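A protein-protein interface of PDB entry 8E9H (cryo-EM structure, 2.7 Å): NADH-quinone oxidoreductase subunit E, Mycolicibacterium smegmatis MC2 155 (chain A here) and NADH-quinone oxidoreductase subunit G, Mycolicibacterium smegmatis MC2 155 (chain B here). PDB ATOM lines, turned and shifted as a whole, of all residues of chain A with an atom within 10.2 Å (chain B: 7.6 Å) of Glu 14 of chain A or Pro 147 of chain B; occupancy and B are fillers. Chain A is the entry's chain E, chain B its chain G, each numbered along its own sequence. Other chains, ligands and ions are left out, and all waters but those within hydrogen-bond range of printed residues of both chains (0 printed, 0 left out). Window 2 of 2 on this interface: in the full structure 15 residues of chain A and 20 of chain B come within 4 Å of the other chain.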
ATOM      1  N   GLU A   7     -23.765 -30.465  -0.614  1.00  0.00           N
ATOM      2  CA  GLU A   7     -24.564 -29.824   0.427  1.00  0.00           C
ATOM      3  C   GLU A   7     -24.582 -30.683   1.697  1.00  0.00           C
ATOM      4  O   GLU A   7     -25.616 -31.183   2.142  1.00  0.00           O
ATOM      5  CB  GLU A   7     -25.986 -29.550  -0.074  1.00  0.00           C
ATOM      6  N   LEU A   8     -23.392 -30.841   2.263  1.00  0.00           N
ATOM      7  CA  LEU A   8     -23.246 -31.615   3.484  1.00  0.00           C
ATOM      8  C   LEU A   8     -23.679 -30.801   4.697  1.00  0.00           C
ATOM      9  O   LEU A   8     -23.789 -29.574   4.647  1.00  0.00           O
ATOM     10  CB  LEU A   8     -21.797 -32.058   3.660  1.00  0.00           C
ATOM     11  CG  LEU A   8     -21.267 -32.999   2.582  1.00  0.00           C
ATOM     12  CD1 LEU A   8     -19.770 -33.147   2.727  1.00  0.00           C
ATOM     13  CD2 LEU A   8     -21.954 -34.346   2.666  1.00  0.00           C
ATOM     14  N   GLY A   9     -23.932 -31.502   5.794  1.00  0.00           N
ATOM     15  CA  GLY A   9     -24.195 -30.857   7.058  1.00  0.00           C
ATOM     16  C   GLY A   9     -25.575 -30.234   7.140  1.00  0.00           C
ATOM     17  O   GLY A   9     -26.450 -30.438   6.297  1.00  0.00           O
ATOM     18  N   GLN A  10     -25.754 -29.445   8.196  1.00  0.00           N
ATOM     19  CA  GLN A  10     -27.042 -28.822   8.463  1.00  0.00           C
ATOM     20  C   GLN A  10     -27.396 -27.824   7.371  1.00  0.00           C
ATOM     21  O   GLN A  10     -26.523 -27.176   6.790  1.00  0.00           O
ATOM     22  CB  GLN A  10     -27.010 -28.116   9.816  1.00  0.00           C
ATOM     23  CG  GLN A  10     -26.575 -28.997  10.962  1.00  0.00           C
ATOM     24  CD  GLN A  10     -26.821 -28.353  12.309  1.00  0.00           C
ATOM     25  OE1 GLN A  10     -27.930 -27.913  12.606  1.00  0.00           O
ATOM     26  NE2 GLN A  10     -25.783 -28.294  13.134  1.00  0.00           N
ATOM     27  N   ARG A  11     -28.689 -27.703   7.094  1.00  0.00           N
ATOM     28  CA  ARG A  11     -29.151 -26.665   6.193  1.00  0.00           C
ATOM     29  C   ARG A  11     -28.971 -25.296   6.851  1.00  0.00           C
ATOM     30  O   ARG A  11     -29.125 -25.161   8.067  1.00  0.00           O
ATOM     31  CB  ARG A  11     -30.617 -26.881   5.830  1.00  0.00           C
ATOM     32  N   PRO A  12     -28.640 -24.263   6.073  1.00  0.00           N
ATOM     33  CA  PRO A  12     -28.368 -22.953   6.686  1.00  0.00           C
ATOM     34  C   PRO A  12     -29.548 -22.365   7.436  1.00  0.00           C
ATOM     35  O   PRO A  12     -29.339 -21.564   8.353  1.00  0.00           O
ATOM     36  CB  PRO A  12     -27.985 -22.079   5.485  1.00  0.00           C
ATOM     37  CG  PRO A  12     -27.584 -23.035   4.423  1.00  0.00           C
ATOM     38  CD  PRO A  12     -28.459 -24.224   4.614  1.00  0.00           C
ATOM     39  N   ASP A  13     -30.777 -22.732   7.085  1.00  0.00           N
ATOM     40  CA  ASP A  13     -31.969 -22.087   7.619  1.00  0.00           C
ATOM     41  C   ASP A  13     -32.521 -22.786   8.854  1.00  0.00           C
ATOM     42  O   ASP A  13     -33.625 -22.456   9.296  1.00  0.00           O
ATOM     43  CB  ASP A  13     -33.050 -22.019   6.540  1.00  0.00           C
ATOM     44  N   GLU A  14     -31.786 -23.736   9.420  1.00  0.00           N
ATOM     45  CA  GLU A  14     -32.296 -24.501  10.544  1.00  0.00           C
ATOM     46  C   GLU A  14     -32.358 -23.647  11.806  1.00  0.00           C
ATOM     47  O   GLU A  14     -31.681 -22.624  11.936  1.00  0.00           O
ATOM     48  CB  GLU A  14     -31.422 -25.726  10.787  1.00  0.00           C
ATOM     49  CG  GLU A  14     -31.476 -26.721   9.657  1.00  0.00           C
ATOM     50  CD  GLU A  14     -30.782 -28.011   9.996  1.00  0.00           C
ATOM     51  OE1 GLU A  14     -30.875 -28.448  11.161  1.00  0.00           O
ATOM     52  OE2 GLU A  14     -30.140 -28.598   9.101  1.00  0.00           O
ATOM     53  N   ALA A  15     -33.185 -24.090  12.748  1.00  0.00           N
ATOM     54  CA  ALA A  15     -33.333 -23.377  14.008  1.00  0.00           C
ATOM     55  C   ALA A  15     -32.012 -23.371  14.762  1.00  0.00           C
ATOM     56  O   ALA A  15     -31.188 -24.276  14.608  1.00  0.00           O
ATOM     57  CB  ALA A  15     -34.423 -24.025  14.861  1.00  0.00           C
ATOM     58  N   GLY A  16     -31.807 -22.341  15.578  1.00  0.00           N
ATOM     59  CA  GLY A  16     -30.550 -22.183  16.264  1.00  0.00           C
ATOM     60  C   GLY A  16     -29.430 -22.136  15.250  1.00  0.00           C
ATOM     61  O   GLY A  16     -28.630 -23.068  15.139  1.00  0.00           O
ATOM     62  N   PRO A  17     -29.362 -21.045  14.491  1.00  0.00           N
ATOM     63  CA  PRO A  17     -28.608 -21.040  13.232  1.00  0.00           C
ATOM     64  C   PRO A  17     -27.322 -21.836  13.346  1.00  0.00           C
ATOM     65  O   PRO A  17     -26.522 -21.610  14.265  1.00  0.00           O
ATOM     66  CB  PRO A  17     -28.323 -19.551  13.005  1.00  0.00           C
ATOM     67  CG  PRO A  17     -29.451 -18.865  13.662  1.00  0.00           C
ATOM     68  CD  PRO A  17     -29.807 -19.693  14.863  1.00  0.00           C
ATOM     69  N   PRO A  18     -27.092 -22.789  12.444  1.00  0.00           N
ATOM     70  CA  PRO A  18     -25.839 -23.544  12.493  1.00  0.00           C
ATOM     71  C   PRO A  18     -24.642 -22.629  12.312  1.00  0.00           C
ATOM     72  O   PRO A  18     -24.729 -21.572  11.684  1.00  0.00           O
ATOM     73  CB  PRO A  18     -25.973 -24.532  11.329  1.00  0.00           C
ATOM     74  CG  PRO A  18     -27.428 -24.641  11.091  1.00  0.00           C
ATOM     75  CD  PRO A  18     -27.992 -23.297  11.397  1.00  0.00           C
ATOM     76  N   ILE A  19     -23.515 -23.043  12.890  1.00  0.00           N
ATOM     77  CA  ILE A  19     -22.289 -22.273  12.758  1.00  0.00           C
ATOM     78  C   ILE A  19     -22.069 -21.942  11.294  1.00  0.00           C
ATOM     79  O   ILE A  19     -22.094 -22.826  10.433  1.00  0.00           O
ATOM     80  CB  ILE A  19     -21.099 -23.057  13.342  1.00  0.00           C
ATOM     81  CG1 ILE A  19     -21.348 -23.420  14.808  1.00  0.00           C
ATOM     82  CG2 ILE A  19     -19.824 -22.254  13.200  1.00  0.00           C
ATOM     83  CD1 ILE A  19     -21.418 -22.234  15.739  1.00  0.00           C
ATOM     84  N   SER A  20     -21.864 -20.662  11.005  1.00  0.00           N
ATOM     85  CA  SER A  20     -21.674 -20.208   9.635  1.00  0.00           C
ATOM     86  C   SER A  20     -20.856 -18.929   9.664  1.00  0.00           C
ATOM     87  O   SER A  20     -20.547 -18.391  10.729  1.00  0.00           O
ATOM     88  CB  SER A  20     -23.015 -19.986   8.933  1.00  0.00           C
ATOM     89  OG  SER A  20     -23.870 -19.181   9.724  1.00  0.00           O
ATOM     90  N   ARG A  96     -24.422 -17.680  17.673  1.00  0.00           N
ATOM     91  CA  ARG A  96     -24.181 -18.209  16.340  1.00  0.00           C
ATOM     92  C   ARG A  96     -24.565 -17.236  15.234  1.00  0.00           C
ATOM     93  O   ARG A  96     -24.696 -17.649  14.078  1.00  0.00           O
ATOM     94  CB  ARG A  96     -24.928 -19.532  16.166  1.00  0.00           C
ATOM     95  CG  ARG A  96     -24.513 -20.584  17.180  1.00  0.00           C
ATOM     96  CD  ARG A  96     -24.716 -21.994  16.664  1.00  0.00           C
ATOM     97  NE  ARG A  96     -26.073 -22.479  16.875  1.00  0.00           N
ATOM     98  CZ  ARG A  96     -26.482 -23.096  17.974  1.00  0.00           C
ATOM     99  NH1 ARG A  96     -25.671 -23.294  19.000  1.00  0.00           N
ATOM    100  NH2 ARG A  96     -27.737 -23.527  18.046  1.00  0.00           N
ATOM    101  N   THR A  97     -24.749 -15.959  15.553  1.00  0.00           N
ATOM    102  CA  THR A  97     -25.025 -14.936  14.559  1.00  0.00           C
ATOM    103  C   THR A  97     -24.336 -13.646  14.969  1.00  0.00           C
ATOM    104  O   THR A  97     -24.032 -13.452  16.151  1.00  0.00           O
ATOM    105  CB  THR A  97     -26.532 -14.685  14.401  1.00  0.00           C
ATOM    106  OG1 THR A  97     -27.124 -14.496  15.690  1.00  0.00           O
ATOM    107  CG2 THR A  97     -27.196 -15.860  13.708  1.00  0.00           C
ATOM    108  N   THR B 145     -39.117 -31.374  14.256  1.00  0.00           N
ATOM    109  CA  THR B 145     -38.839 -31.604  12.850  1.00  0.00           C
ATOM    110  C   THR B 145     -37.485 -31.017  12.477  1.00  0.00           C
ATOM    111  O   THR B 145     -37.068 -29.986  13.007  1.00  0.00           O
ATOM    112  CB  THR B 145     -39.934 -31.003  11.962  1.00  0.00           C
ATOM    113  OG1 THR B 145     -39.579 -31.162  10.585  1.00  0.00           O
ATOM    114  CG2 THR B 145     -40.122 -29.530  12.266  1.00  0.00           C
ATOM    115  N   PHE B 146     -36.811 -31.696  11.556  1.00  0.00           N
ATOM    116  CA  PHE B 146     -35.534 -31.287  11.002  1.00  0.00           C
ATOM    117  C   PHE B 146     -35.603 -31.437   9.492  1.00  0.00           C
ATOM    118  O   PHE B 146     -36.374 -32.262   8.989  1.00  0.00           O
ATOM    119  CB  PHE B 146     -34.371 -32.145  11.521  1.00  0.00           C
ATOM    120  CG  PHE B 146     -34.095 -31.986  12.980  1.00  0.00           C
ATOM    121  CD1 PHE B 146     -33.362 -30.916  13.445  1.00  0.00           C
ATOM    122  CD2 PHE B 146     -34.553 -32.920  13.884  1.00  0.00           C
ATOM    123  CE1 PHE B 146     -33.101 -30.775  14.787  1.00  0.00           C
ATOM    124  CE2 PHE B 146     -34.296 -32.784  15.226  1.00  0.00           C
ATOM    125  CZ  PHE B 146     -33.569 -31.711  15.679  1.00  0.00           C
ATOM    126  N   PRO B 147     -34.820 -30.664   8.746  1.00  0.00           N
ATOM    127  CA  PRO B 147     -34.657 -30.974   7.326  1.00  0.00           C
ATOM    128  C   PRO B 147     -34.076 -32.367   7.162  1.00  0.00           C
ATOM    129  O   PRO B 147     -33.123 -32.745   7.846  1.00  0.00           O
ATOM    130  CB  PRO B 147     -33.692 -29.892   6.833  1.00  0.00           C
ATOM    131  CG  PRO B 147     -33.833 -28.789   7.804  1.00  0.00           C
ATOM    132  CD  PRO B 147     -34.115 -29.430   9.122  1.00  0.00           C
ATOM    133  N   LYS B 148     -34.659 -33.136   6.253  1.00  0.00           N
ATOM    134  CA  LYS B 148     -34.234 -34.506   6.037  1.00  0.00           C
ATOM    135  C   LYS B 148     -34.286 -34.826   4.552  1.00  0.00           C
ATOM    136  O   LYS B 148     -35.131 -34.284   3.831  1.00  0.00           O
ATOM    137  CB  LYS B 148     -35.123 -35.500   6.800  1.00  0.00           C
ATOM    138  CG  LYS B 148     -36.539 -35.621   6.253  1.00  0.00           C
ATOM    139  CD  LYS B 148     -37.258 -36.829   6.814  1.00  0.00           C
ATOM    140  CE  LYS B 148     -37.752 -36.579   8.215  1.00  0.00           C
ATOM    141  NZ  LYS B 148     -38.204 -37.832   8.866  1.00  0.00           N
ATOM    142  N   PRO B 149     -33.394 -35.699   4.064  1.00  0.00           N
ATOM    143  CA  PRO B 149     -32.209 -36.245   4.722  1.00  0.00           C
ATOM    144  C   PRO B 149     -30.977 -35.427   4.381  1.00  0.00           C
ATOM    145  O   PRO B 149     -30.762 -35.144   3.205  1.00  0.00           O
ATOM    146  CB  PRO B 149     -32.110 -37.645   4.136  1.00  0.00           C
ATOM    147  CG  PRO B 149     -32.611 -37.478   2.758  1.00  0.00           C
ATOM    148  CD  PRO B 149     -33.664 -36.399   2.798  1.00  0.00           C
ATOM    149  N   ILE B 150     -30.194 -35.051   5.364  1.00  0.00           N
ATOM    150  CA  ILE B 150     -28.959 -34.322   5.113  1.00  0.00           C
ATOM    151  C   ILE B 150     -27.829 -35.325   4.974  1.00  0.00           C
ATOM    152  O   ILE B 150     -27.834 -36.389   5.596  1.00  0.00           O
ATOM    153  CB  ILE B 150     -28.670 -33.297   6.226  1.00  0.00           C
ATOM    154  CG1 ILE B 150     -28.542 -33.988   7.582  1.00  0.00           C
ATOM    155  CG2 ILE B 150     -29.767 -32.254   6.273  1.00  0.00           C
ATOM    156  CD1 ILE B 150     -27.811 -33.164   8.600  1.00  0.00           C
ATOM    157  N   LEU B 158     -28.362 -38.795   6.698  1.00  0.00           N
ATOM    158  CA  LEU B 158     -28.746 -38.650   8.096  1.00  0.00           C
ATOM    159  C   LEU B 158     -30.129 -38.023   8.152  1.00  0.00           C
ATOM    160  O   LEU B 158     -30.334 -36.921   7.634  1.00  0.00           O
ATOM    161  CB  LEU B 158     -27.726 -37.804   8.850  1.00  0.00           C
ATOM    162  CG  LEU B 158     -28.173 -37.255  10.198  1.00  0.00           C
ATOM    163  CD1 LEU B 158     -28.543 -38.382  11.133  1.00  0.00           C
ATOM    164  CD2 LEU B 158     -27.075 -36.407  10.788  1.00  0.00           C
ATOM    165  N   ASP B 159     -31.075 -38.724   8.772  1.00  0.00           N
ATOM    166  CA  ASP B 159     -32.431 -38.216   8.964  1.00  0.00           C
ATOM    167  C   ASP B 159     -32.619 -37.951  10.449  1.00  0.00           C
ATOM    168  O   ASP B 159     -33.076 -38.819  11.194  1.00  0.00           O
ATOM    169  CB  ASP B 159     -33.460 -39.210   8.444  1.00  0.00           C
ATOM    170  CG  ASP B 159     -34.875 -38.726   8.638  1.00  0.00           C
ATOM    171  OD1 ASP B 159     -35.052 -37.536   8.963  1.00  0.00           O
ATOM    172  OD2 ASP B 159     -35.811 -39.530   8.473  1.00  0.00           O
ATOM    173  N   ARG B 160     -32.282 -36.738  10.881  1.00  0.00           N
ATOM    174  CA  ARG B 160     -32.197 -36.460  12.309  1.00  0.00           C
ATOM    175  C   ARG B 160     -33.524 -36.646  13.023  1.00  0.00           C
ATOM    176  O   ARG B 160     -33.529 -36.919  14.226  1.00  0.00           O
ATOM    177  CB  ARG B 160     -31.690 -35.043  12.532  1.00  0.00           C
ATOM    178  CG  ARG B 160     -30.231 -34.877  12.205  1.00  0.00           C
ATOM    179  CD  ARG B 160     -29.882 -33.432  12.012  1.00  0.00           C
ATOM    180  NE  ARG B 160     -30.512 -32.885  10.820  1.00  0.00           N
ATOM    181  CZ  ARG B 160     -30.457 -31.609  10.475  1.00  0.00           C
ATOM    182  NH1 ARG B 160     -29.802 -30.727  11.206  1.00  0.00           N
ATOM    183  NH2 ARG B 160     -31.072 -31.211   9.366  1.00  0.00           N
ATOM    184  N   GLU B 161     -34.648 -36.503  12.324  1.00  0.00           N
ATOM    185  CA  GLU B 161     -35.929 -36.667  12.996  1.00  0.00           C
ATOM    186  C   GLU B 161     -36.086 -38.073  13.551  1.00  0.00           C
ATOM    187  O   GLU B 161     -36.624 -38.247  14.649  1.00  0.00           O
ATOM    188  CB  GLU B 161     -37.074 -36.347  12.043  1.00  0.00           C
ATOM    189  CG  GLU B 161     -36.950 -35.018  11.349  1.00  0.00           C
ATOM    190  CD  GLU B 161     -38.234 -34.609  10.661  1.00  0.00           C
ATOM    191  OE1 GLU B 161     -39.128 -35.465  10.516  1.00  0.00           O
ATOM    192  OE2 GLU B 161     -38.351 -33.430  10.267  1.00  0.00           O
ATOM    193  N   GLU B 186     -25.597 -29.386  19.322  1.00  0.00           N
ATOM    194  CA  GLU B 186     -26.736 -28.720  19.942  1.00  0.00           C
ATOM    195  C   GLU B 186     -27.019 -29.281  21.328  1.00  0.00           C
ATOM    196  O   GLU B 186     -26.230 -30.067  21.860  1.00  0.00           O
ATOM    197  CB  GLU B 186     -27.977 -28.850  19.060  1.00  0.00           C
ATOM    198  CG  GLU B 186     -27.801 -28.318  17.656  1.00  0.00           C
ATOM    199  CD  GLU B 186     -27.680 -26.813  17.619  1.00  0.00           C
ATOM    200  OE1 GLU B 186     -27.928 -26.170  18.660  1.00  0.00           O
ATOM    201  OE2 GLU B 186     -27.345 -26.268  16.546  1.00  0.00           O
ATOM    202  N   LEU B 190     -33.103 -30.132  20.764  1.00  0.00           N
ATOM    203  CA  LEU B 190     -32.443 -29.810  19.511  1.00  0.00           C
ATOM    204  C   LEU B 190     -31.170 -30.612  19.293  1.00  0.00           C
ATOM    205  O   LEU B 190     -30.554 -30.483  18.232  1.00  0.00           O
ATOM    206  CB  LEU B 190     -32.123 -28.316  19.471  1.00  0.00           C
ATOM    207  CG  LEU B 190     -31.771 -27.724  18.108  1.00  0.00           C
ATOM    208  CD1 LEU B 190     -32.942 -27.838  17.154  1.00  0.00           C
ATOM    209  CD2 LEU B 190     -31.344 -26.275  18.261  1.00  0.00           C
ATOM    210  N   GLN B 192     -28.569 -33.236  18.129  1.00  0.00           N
ATOM    211  CA  GLN B 192     -28.627 -33.948  16.863  1.00  0.00           C
ATOM    212  C   GLN B 192     -27.231 -34.371  16.448  1.00  0.00           C
ATOM    213  O   GLN B 192     -26.295 -33.584  16.512  1.00  0.00           O
ATOM    214  CB  GLN B 192     -29.234 -33.066  15.774  1.00  0.00           C
ATOM    215  CG  GLN B 192     -28.407 -31.830  15.501  1.00  0.00           C
ATOM    216  CD  GLN B 192     -29.162 -30.783  14.731  1.00  0.00           C
ATOM    217  OE1 GLN B 192     -29.014 -30.664  13.517  1.00  0.00           O
ATOM    218  NE2 GLN B 192     -29.982 -30.013  15.429  1.00  0.00           N
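The side-chain carboxylate of Glu 14 of chain A lies within salt-bridge range of the guanidinium group of Arg 160 of chain B.
The side-chain carboxylate (OE1) of Glu 186 of chain B is in salt-bridge range of the guanidinium group (NH2) of Arg 96 of chain A, at 2.7 Å.
OE1 of Gln 10 of chain A sits close to OE1 of Gln 192 of chain B.
The backbone carbonyl oxygen of Pro 147 of chain B sits at hydrogen-bond distance from the guanidinium group of Arg 160 of chain B.
The side-chain amide oxygen (OE1) of Gln 10 of chain A sits close to the side-chain carboxylate (OE1) of Glu 14 of chain A (3.3 Å).
N of Leu 158 of chain B lies within hydrogen-bond range of O of Ile 150 of chain B, 2.7 Å away.
N of Arg 11 of chain A sits at hydrogen-bond distance from OE2 of Glu 14 of chain A, at 2.6 Å.
O of Pro 17 of chain A is in hydrogen-bond range of NE of Arg 96 of chain A, 2.8 Å away.
NH1 of Arg 160 of chain B sits at hydrogen-bond distance from OE1 of Gln 192 of chain B (2.4 Å).
Gly 9 of chain A touches Ile 150 of chain B.
Gln 10 of chain A touches Arg 160 of chain B.
Pro 147 of chain B touches Glu 14 of chain A (CG to CG, 3.6 Å).
OE1 of Glu 14 of chain A touches OE1 of Gln 192 of chain B (3.7 Å).
OE2 of Glu 186 of chain B touches O of Gly 16 of chain A, at 3.7 Å.
Glu 14 of chain A touches just these residues of chain B: Pro 147 (3.6 Å), Arg 160 (2.5 Å) and Gln 192 (3.7 Å).
Of chain A, only Glu 14 (3.6 Å) comes within 4 Å of Pro 147 of chain B.
Of the printed residues of chain A, Gln 192 of chain B touches Gln 10 (3.1 Å) and Glu 14 (3.7 Å).
Of the printed residues of chain B, Gly 16 of chain A touches Glu 186 (3.7 Å).
Of the printed residues of chain B, Arg 96 of chain A touches Glu 186 (2.7 Å).
Printed residues of chain A within 4 Å of Ile 150 of chain B: Gly 9 (3.6 Å).
Of the printed residues of chain A, Arg 160 of chain B touches Gln 10 and Glu 14.
Pro 12 of chain A touches none of the printed residues of chain B.
Asp 159 of chain B touches none of the printed residues of chain A.
The nearest printed residue of chain A that does not touch Arg 160 of chain B is Arg 11 of chain A (4.8 Å).
Among the printed residues, 8 pairs touch across the chains.
Among the printed residues, Asp or Glu carboxylates within 4 Å of a Lys or Arg side-chain nitrogen of the other chain: Glu 14 of chain A with Arg 160 of chain B (2.5 Å) and Arg 96 of chain A with Glu 186 of chain B (2.7 Å).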
